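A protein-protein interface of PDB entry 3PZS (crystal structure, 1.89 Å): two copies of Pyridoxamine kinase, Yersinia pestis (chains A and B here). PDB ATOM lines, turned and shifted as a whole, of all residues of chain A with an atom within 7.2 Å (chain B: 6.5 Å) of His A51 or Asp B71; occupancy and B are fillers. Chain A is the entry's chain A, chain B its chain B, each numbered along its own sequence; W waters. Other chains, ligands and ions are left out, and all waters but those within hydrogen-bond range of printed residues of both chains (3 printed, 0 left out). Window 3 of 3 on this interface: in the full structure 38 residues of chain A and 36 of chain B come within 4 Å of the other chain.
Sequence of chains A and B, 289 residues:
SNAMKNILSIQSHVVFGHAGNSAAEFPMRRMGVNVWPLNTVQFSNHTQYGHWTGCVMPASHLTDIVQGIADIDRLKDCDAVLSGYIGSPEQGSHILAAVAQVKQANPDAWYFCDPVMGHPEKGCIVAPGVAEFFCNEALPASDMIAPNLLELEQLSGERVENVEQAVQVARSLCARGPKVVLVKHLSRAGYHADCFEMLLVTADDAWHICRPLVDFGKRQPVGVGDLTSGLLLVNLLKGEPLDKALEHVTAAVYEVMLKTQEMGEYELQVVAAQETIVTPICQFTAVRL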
ATOM      1  N   SER A  44     -15.451  -6.886   7.917  1.00  0.00           N
ATOM      2  CA  SER A  44     -16.364  -6.511   6.834  1.00  0.00           C
ATOM      3  C   SER A  44     -17.669  -5.957   7.379  1.00  0.00           C
ATOM      4  O   SER A  44     -18.275  -5.074   6.764  1.00  0.00           O
ATOM      5  CB  SER A  44     -16.675  -7.727   5.967  1.00  0.00           C
ATOM      6  OG  SER A  44     -17.195  -8.776   6.771  1.00  0.00           O
ATOM      7  N   ASN A  45     -18.099  -6.491   8.525  1.00  0.00           N
ATOM      8  CA  ASN A  45     -19.355  -6.149   9.209  1.00  0.00           C
ATOM      9  C   ASN A  45     -19.285  -6.676  10.636  1.00  0.00           C
ATOM     10  O   ASN A  45     -18.368  -7.463  10.943  1.00  0.00           O
ATOM     11  CB  ASN A  45     -20.538  -6.767   8.441  1.00  0.00           C
ATOM     12  CG  ASN A  45     -20.359  -8.249   8.238  1.00  0.00           C
ATOM     13  OD1 ASN A  45     -19.841  -8.700   7.211  1.00  0.00           O
ATOM     14  ND2 ASN A  45     -20.674  -9.026   9.270  1.00  0.00           N
ATOM     15  N   HIS A  46     -20.207  -6.243  11.525  1.00  0.00           N
ATOM     16  CA  HIS A  46     -20.149  -6.691  12.921  1.00  0.00           C
ATOM     17  C   HIS A  46     -20.493  -8.190  13.005  1.00  0.00           C
ATOM     18  O   HIS A  46     -21.055  -8.754  12.062  1.00  0.00           O
ATOM     19  CB  HIS A  46     -21.008  -5.825  13.885  1.00  0.00           C
ATOM     20  CG  HIS A  46     -22.481  -5.826  13.597  1.00  0.00           C
ATOM     21  ND1 HIS A  46     -23.248  -6.976  13.751  1.00  0.00           N
ATOM     22  CD2 HIS A  46     -23.295  -4.796  13.260  1.00  0.00           C
ATOM     23  CE1 HIS A  46     -24.488  -6.623  13.443  1.00  0.00           C
ATOM     24  NE2 HIS A  46     -24.567  -5.311  13.154  1.00  0.00           N
ATOM     25  N   THR A  47     -20.084  -8.832  14.101  1.00  0.00           N
ATOM     26  CA  THR A  47     -20.213 -10.283  14.284  1.00  0.00           C
ATOM     27  C   THR A  47     -21.650 -10.771  14.504  1.00  0.00           C
ATOM     28  O   THR A  47     -21.880 -11.975  14.383  1.00  0.00           O
ATOM     29  CB  THR A  47     -19.332 -10.741  15.462  1.00  0.00           C
ATOM     30  OG1 THR A  47     -19.839 -10.158  16.668  1.00  0.00           O
ATOM     31  CG2 THR A  47     -17.868 -10.372  15.272  1.00  0.00           C
ATOM     32  N   GLN A  48     -22.615  -9.872  14.774  1.00  0.00           N
ATOM     33  CA  GLN A  48     -24.000 -10.297  15.034  1.00  0.00           C
ATOM     34  C   GLN A  48     -24.724 -10.684  13.742  1.00  0.00           C
ATOM     35  O   GLN A  48     -25.792 -11.303  13.803  1.00  0.00           O
ATOM     36  CB  GLN A  48     -24.783  -9.294  15.882  1.00  0.00           C
ATOM     37  CG  GLN A  48     -24.241  -9.252  17.327  1.00  0.00           C
ATOM     38  CD  GLN A  48     -25.132  -8.540  18.327  1.00  0.00           C
ATOM     39  OE1 GLN A  48     -26.368  -8.623  18.295  1.00  0.00           O
ATOM     40  NE2 GLN A  48     -24.516  -7.837  19.265  1.00  0.00           N
ATOM     41  N   TYR A  49     -24.086 -10.471  12.572  1.00  0.00           N
ATOM     42  CA  TYR A  49     -24.612 -11.015  11.317  1.00  0.00           C
ATOM     43  C   TYR A  49     -24.473 -12.553  11.333  1.00  0.00           C
ATOM     44  O   TYR A  49     -25.169 -13.233  10.584  1.00  0.00           O
ATOM     45  CB  TYR A  49     -23.874 -10.438  10.094  1.00  0.00           C
ATOM     46  CG  TYR A  49     -24.355  -9.057   9.708  1.00  0.00           C
ATOM     47  CD1 TYR A  49     -23.785  -7.920  10.273  1.00  0.00           C
ATOM     48  CD2 TYR A  49     -25.382  -8.886   8.785  1.00  0.00           C
ATOM     49  CE1 TYR A  49     -24.235  -6.648   9.947  1.00  0.00           C
ATOM     50  CE2 TYR A  49     -25.834  -7.612   8.437  1.00  0.00           C
ATOM     51  CZ  TYR A  49     -25.258  -6.494   9.031  1.00  0.00           C
ATOM     52  OH  TYR A  49     -25.682  -5.231   8.734  1.00  0.00           O
ATOM     53  N   GLY A  50     -23.558 -13.058  12.175  1.00  0.00           N
ATOM     54  CA  GLY A  50     -23.275 -14.483  12.356  1.00  0.00           C
ATOM     55  C   GLY A  50     -22.059 -14.965  11.584  1.00  0.00           C
ATOM     56  O   GLY A  50     -21.644 -16.121  11.706  1.00  0.00           O
ATOM     57  N   HIS A  51     -21.502 -14.071  10.753  1.00  0.00           N
ATOM     58  CA  HIS A  51     -20.321 -14.306   9.943  1.00  0.00           C
ATOM     59  C   HIS A  51     -19.758 -12.973   9.501  1.00  0.00           C
ATOM     60  O   HIS A  51     -20.498 -11.994   9.391  1.00  0.00           O
ATOM     61  CB  HIS A  51     -20.604 -15.213   8.734  1.00  0.00           C
ATOM     62  CG  HIS A  51     -21.736 -14.763   7.870  1.00  0.00           C
ATOM     63  ND1 HIS A  51     -21.515 -14.064   6.713  1.00  0.00           N
ATOM     64  CD2 HIS A  51     -23.064 -14.996   7.995  1.00  0.00           C
ATOM     65  CE1 HIS A  51     -22.711 -13.854   6.185  1.00  0.00           C
ATOM     66  NE2 HIS A  51     -23.675 -14.392   6.932  1.00  0.00           N
ATOM     67  N   TRP A  52     -18.446 -12.947   9.240  1.00  0.00           N
ATOM     68  CA  TRP A  52     -17.723 -11.742   8.800  1.00  0.00           C
ATOM     69  C   TRP A  52     -16.369 -12.156   8.241  1.00  0.00           C
ATOM     70  O   TRP A  52     -15.954 -13.286   8.457  1.00  0.00           O
ATOM     71  CB  TRP A  52     -17.530 -10.783  10.014  1.00  0.00           C
ATOM     72  CG  TRP A  52     -16.610 -11.315  11.081  1.00  0.00           C
ATOM     73  CD1 TRP A  52     -15.279 -11.048  11.216  1.00  0.00           C
ATOM     74  CD2 TRP A  52     -16.940 -12.247  12.136  1.00  0.00           C
ATOM     75  NE1 TRP A  52     -14.763 -11.734  12.291  1.00  0.00           N
ATOM     76  CE2 TRP A  52     -15.763 -12.467  12.881  1.00  0.00           C
ATOM     77  CE3 TRP A  52     -18.130 -12.885  12.545  1.00  0.00           C
ATOM     78  CZ2 TRP A  52     -15.733 -13.306  14.007  1.00  0.00           C
ATOM     79  CZ3 TRP A  52     -18.100 -13.720  13.655  1.00  0.00           C
ATOM     80  CH2 TRP A  52     -16.913 -13.929  14.369  1.00  0.00           C
ATOM     81  N   THR A  53     -15.665 -11.232   7.585  1.00  0.00           N
ATOM     82  CA  THR A  53     -14.287 -11.405   7.119  1.00  0.00           C
ATOM     83  C   THR A  53     -13.459 -10.263   7.720  1.00  0.00           C
ATOM     84  O   THR A  53     -14.026  -9.314   8.275  1.00  0.00           O
ATOM     85  CB  THR A  53     -14.191 -11.424   5.602  1.00  0.00           C
ATOM     86  OG1 THR A  53     -14.563 -10.127   5.122  1.00  0.00           O
ATOM     87  CG2 THR A  53     -15.040 -12.542   4.949  1.00  0.00           C
ATOM     88  N   ASP B  64     -10.731  -9.703   0.805  1.00  0.00           N
ATOM     89  CA  ASP B  64     -11.439 -10.452   1.837  1.00  0.00           C
ATOM     90  C   ASP B  64     -12.599  -9.634   2.397  1.00  0.00           C
ATOM     91  O   ASP B  64     -13.683 -10.122   2.508  1.00  0.00           O
ATOM     92  CB  ASP B  64     -10.543 -10.773   3.038  1.00  0.00           C
ATOM     93  CG  ASP B  64      -9.496 -11.834   2.777  1.00  0.00           C
ATOM     94  OD1 ASP B  64      -9.492 -12.480   1.733  1.00  0.00           O
ATOM     95  OD2 ASP B  64      -8.617 -11.978   3.645  1.00  0.00           O
ATOM     96  N   VAL B  66     -14.222  -7.150   0.938  1.00  0.00           N
ATOM     97  CA  VAL B  66     -15.236  -6.988  -0.110  1.00  0.00           C
ATOM     98  C   VAL B  66     -16.086  -8.266  -0.199  1.00  0.00           C
ATOM     99  O   VAL B  66     -17.300  -8.161  -0.291  1.00  0.00           O
ATOM    100  CB  VAL B  66     -14.600  -6.573  -1.468  1.00  0.00           C
ATOM    101  CG1 VAL B  66     -15.650  -6.506  -2.573  1.00  0.00           C
ATOM    102  CG2 VAL B  66     -13.918  -5.210  -1.331  1.00  0.00           C
ATOM    103  N   GLN B  67     -15.454  -9.452  -0.110  1.00  0.00           N
ATOM    104  CA  GLN B  67     -16.196 -10.722  -0.098  1.00  0.00           C
ATOM    105  C   GLN B  67     -17.127 -10.780   1.117  1.00  0.00           C
ATOM    106  O   GLN B  67     -18.253 -11.228   0.985  1.00  0.00           O
ATOM    107  CB  GLN B  67     -15.258 -11.951  -0.106  1.00  0.00           C
ATOM    108  CG  GLN B  67     -16.038 -13.284  -0.320  1.00  0.00           C
ATOM    109  CD  GLN B  67     -16.889 -13.252  -1.565  1.00  0.00           C
ATOM    110  OE1 GLN B  67     -16.415 -12.916  -2.651  1.00  0.00           O
ATOM    111  NE2 GLN B  67     -18.165 -13.628  -1.442  1.00  0.00           N
ATOM    112  N   GLY B  68     -16.664 -10.299   2.267  1.00  0.00           N
ATOM    113  CA  GLY B  68     -17.492 -10.291   3.467  1.00  0.00           C
ATOM    114  C   GLY B  68     -18.751  -9.462   3.305  1.00  0.00           C
ATOM    115  O   GLY B  68     -19.831  -9.863   3.760  1.00  0.00           O
ATOM    116  N   ILE B  69     -18.627  -8.300   2.633  1.00  0.00           N
ATOM    117  CA  ILE B  69     -19.784  -7.416   2.398  1.00  0.00           C
ATOM    118  C   ILE B  69     -20.720  -8.103   1.396  1.00  0.00           C
ATOM    119  O   ILE B  69     -21.941  -8.025   1.556  1.00  0.00           O
ATOM    120  CB  ILE B  69     -19.358  -5.995   1.935  1.00  0.00           C
ATOM    121  CG1 ILE B  69     -18.409  -5.362   2.987  1.00  0.00           C
ATOM    122  CG2 ILE B  69     -20.605  -5.088   1.682  1.00  0.00           C
ATOM    123  CD1 ILE B  69     -17.765  -3.940   2.542  1.00  0.00           C
ATOM    124  N   ALA B  70     -20.157  -8.836   0.419  1.00  0.00           N
ATOM    125  CA  ALA B  70     -20.998  -9.584  -0.534  1.00  0.00           C
ATOM    126  C   ALA B  70     -21.726 -10.751   0.192  1.00  0.00           C
ATOM    127  O   ALA B  70     -22.890 -10.999  -0.096  1.00  0.00           O
ATOM    128  CB  ALA B  70     -20.151 -10.110  -1.675  1.00  0.00           C
ATOM    129  N   ASP B  71     -21.070 -11.368   1.214  1.00  0.00           N
ATOM    130  CA  ASP B  71     -21.613 -12.479   2.017  1.00  0.00           C
ATOM    131  C   ASP B  71     -22.860 -12.075   2.822  1.00  0.00           C
ATOM    132  O   ASP B  71     -23.683 -12.934   3.118  1.00  0.00           O
ATOM    133  CB  ASP B  71     -20.532 -13.045   2.962  1.00  0.00           C
ATOM    134  CG  ASP B  71     -19.420 -13.837   2.280  1.00  0.00           C
ATOM    135  OD1 ASP B  71     -19.599 -14.234   1.095  1.00  0.00           O
ATOM    136  OD2 ASP B  71     -18.387 -14.088   2.933  1.00  0.00           O
ATOM    137  N   ILE B  72     -23.015 -10.787   3.169  1.00  0.00           N
ATOM    138  CA  ILE B  72     -24.220 -10.330   3.859  1.00  0.00           C
ATOM    139  C   ILE B  72     -25.195  -9.666   2.844  1.00  0.00           C
ATOM    140  O   ILE B  72     -26.143  -8.999   3.265  1.00  0.00           O
ATOM    141  CB  ILE B  72     -23.910  -9.420   5.090  1.00  0.00           C
ATOM    142  CG1 ILE B  72     -23.108  -8.134   4.715  1.00  0.00           C
ATOM    143  CG2 ILE B  72     -23.224 -10.228   6.174  1.00  0.00           C
ATOM    144  CD1 ILE B  72     -23.155  -7.055   5.798  1.00  0.00           C
ATOM    145  N   ASP B  73     -24.958  -9.881   1.525  1.00  0.00           N
ATOM    146  CA  ASP B  73     -25.728  -9.368   0.371  1.00  0.00           C
ATOM    147  C   ASP B  73     -25.918  -7.841   0.425  1.00  0.00           C
ATOM    148  O   ASP B  73     -26.984  -7.325   0.076  1.00  0.00           O
ATOM    149  CB  ASP B  73     -27.087 -10.083   0.206  1.00  0.00           C
ATOM    150  CG  ASP B  73     -27.669 -10.041  -1.208  1.00  0.00           C
ATOM    151  OD1 ASP B  73     -27.010  -9.463  -2.116  1.00  0.00           O
ATOM    152  OD2 ASP B  73     -28.778 -10.582  -1.408  1.00  0.00           O
ATOM    153  N   ARG B  74     -24.865  -7.119   0.839  1.00  0.00           N
ATOM    154  CA  ARG B  74     -24.911  -5.654   0.904  1.00  0.00           C
ATOM    155  C   ARG B  74     -24.001  -4.988  -0.119  1.00  0.00           C
ATOM    156  O   ARG B  74     -24.091  -3.764  -0.293  1.00  0.00           O
ATOM    157  CB  ARG B  74     -24.578  -5.158   2.323  1.00  0.00           C
ATOM    158  CG  ARG B  74     -25.711  -5.377   3.323  1.00  0.00           C
ATOM    159  CD  ARG B  74     -26.949  -4.545   3.036  1.00  0.00           C
ATOM    160  NE  ARG B  74     -27.856  -4.513   4.181  1.00  0.00           N
ATOM    161  CZ  ARG B  74     -28.942  -3.751   4.260  1.00  0.00           C
ATOM    162  NH1 ARG B  74     -29.272  -2.943   3.259  1.00  0.00           N
ATOM    163  NH2 ARG B  74     -29.705  -3.785   5.343  1.00  0.00           N
ATOM    164  N   LEU B  75     -23.165  -5.769  -0.847  1.00  0.00           N
ATOM    165  CA  LEU B  75     -22.260  -5.174  -1.823  1.00  0.00           C
ATOM    166  C   LEU B  75     -23.035  -4.489  -2.972  1.00  0.00           C
ATOM    167  O   LEU B  75     -22.560  -3.486  -3.509  1.00  0.00           O
ATOM    168  CB  LEU B  75     -21.250  -6.202  -2.361  1.00  0.00           C
ATOM    169  CG  LEU B  75     -20.009  -5.601  -3.015  1.00  0.00           C
ATOM    170  CD1 LEU B  75     -19.095  -4.943  -1.962  1.00  0.00           C
ATOM    171  CD2 LEU B  75     -19.251  -6.651  -3.810  1.00  0.00           C
HETATM  172  O   HOH W   1     -27.678  -4.675   7.097  1.00  0.00           O
HETATM  173  O   HOH W   2     -18.608 -13.688   5.725  1.00  0.00           O
HETATM  174  O   HOH W   3     -19.845 -11.296   6.068  1.00  0.00           O
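The backbone carbonyl oxygen (O) of Ile B69 is in hydrogen-bond range of the backbone NH (N) of Arg B74, 3.1 Å away. The side-chain hydroxyl of Ser A44 lies within hydrogen-bond range of the side-chain amide oxygen of Asn A45, 2.7 Å away. The side-chain amide nitrogen of Asn A45 sits at hydrogen-bond distance from the backbone carbonyl oxygen of His A51. N of Ser A44 lies within hydrogen-bond range of O of Thr A53 (2.8 Å). NE2 of Gln B67 lies within hydrogen-bond range of OD1 of Asp B71 (3.0 Å).
No position is printed for both chains.
His A51 touches just these residues of chain B: Asp B71 (3.3 Å) and Ile B72 (3.7 Å). Of chain A, only His A51 comes within 4 Å of Asp B71. Printed residues of chain A within 4 Å of Gly B68: Ser A44 (3.6 Å), Asn A45 (3.6 Å) and Thr A53 (3.4 Å). Printed residues of chain A within 4 Å of Asp B64: Thr A53. Of the printed residues of chain B, Asn A45 touches Gly B68 (3.6 Å) and Ile B72 (3.7 Å). His A46 touches none of the printed residues of chain B. The nearest residue of chain A that does not touch Asp B71 is Thr A53 (4.2 Å). The nearest printed residue of chain B that does not touch Ser A44 is Asp B64 (5.2 Å).
Hydrophobic or aromatic side chains of chain B within 4 Å of the printed part of chain A: Ile B69 and Ile B72. Of the 10 printed residues of chain A, 5 touch a printed residue of chain B. Printed residues of chain A that touch a printed residue of chain B: Ser A44, Asn A45, Tyr A49, His A51 and Thr A53. Hydrophobic or aromatic side chains of chain A within 4 Å of the printed part of chain B: Tyr A49 and His A51. Among the printed residues, 9 pairs touch across the chains.
O of Asp B64 sits at hydrogen-bond distance from OG1 of Thr A53 (2.8 Å).
OG of Ser A44 touches CA of Gly B68, at 3.6 Å. Ser A44 touches Ile B69. Gly B68 touches Asn A45 (O to OD1, 3.6 Å). Asn A45 touches Ile B72. Tyr A49 touches Ile B72. O of Asp B71 touches CE1 of His A51 (3.3 Å). Ile B72 touches His A51 (CG2 to CE1, 3.7 Å). CA of Gly B68 touches OG1 of Thr A53, 3.4 Å away.
Water W1 lies within hydrogen-bond range of the side-chain hydroxyl of Tyr A49 (2.6 Å) and the guanidinium group of Arg B74 (2.8 Å). Water W3 lies within hydrogen-bond range of the backbone carbonyl oxygen of Gly B68, the side-chain amide oxygen of Asn A45 and a ring nitrogen (ND1) of His A51. Water W2 lies within hydrogen-bond range of the side-chain carboxylate of Asp B71 (2.8 Å) and a ring nitrogen (ND1) of His A51 (3.1 Å).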
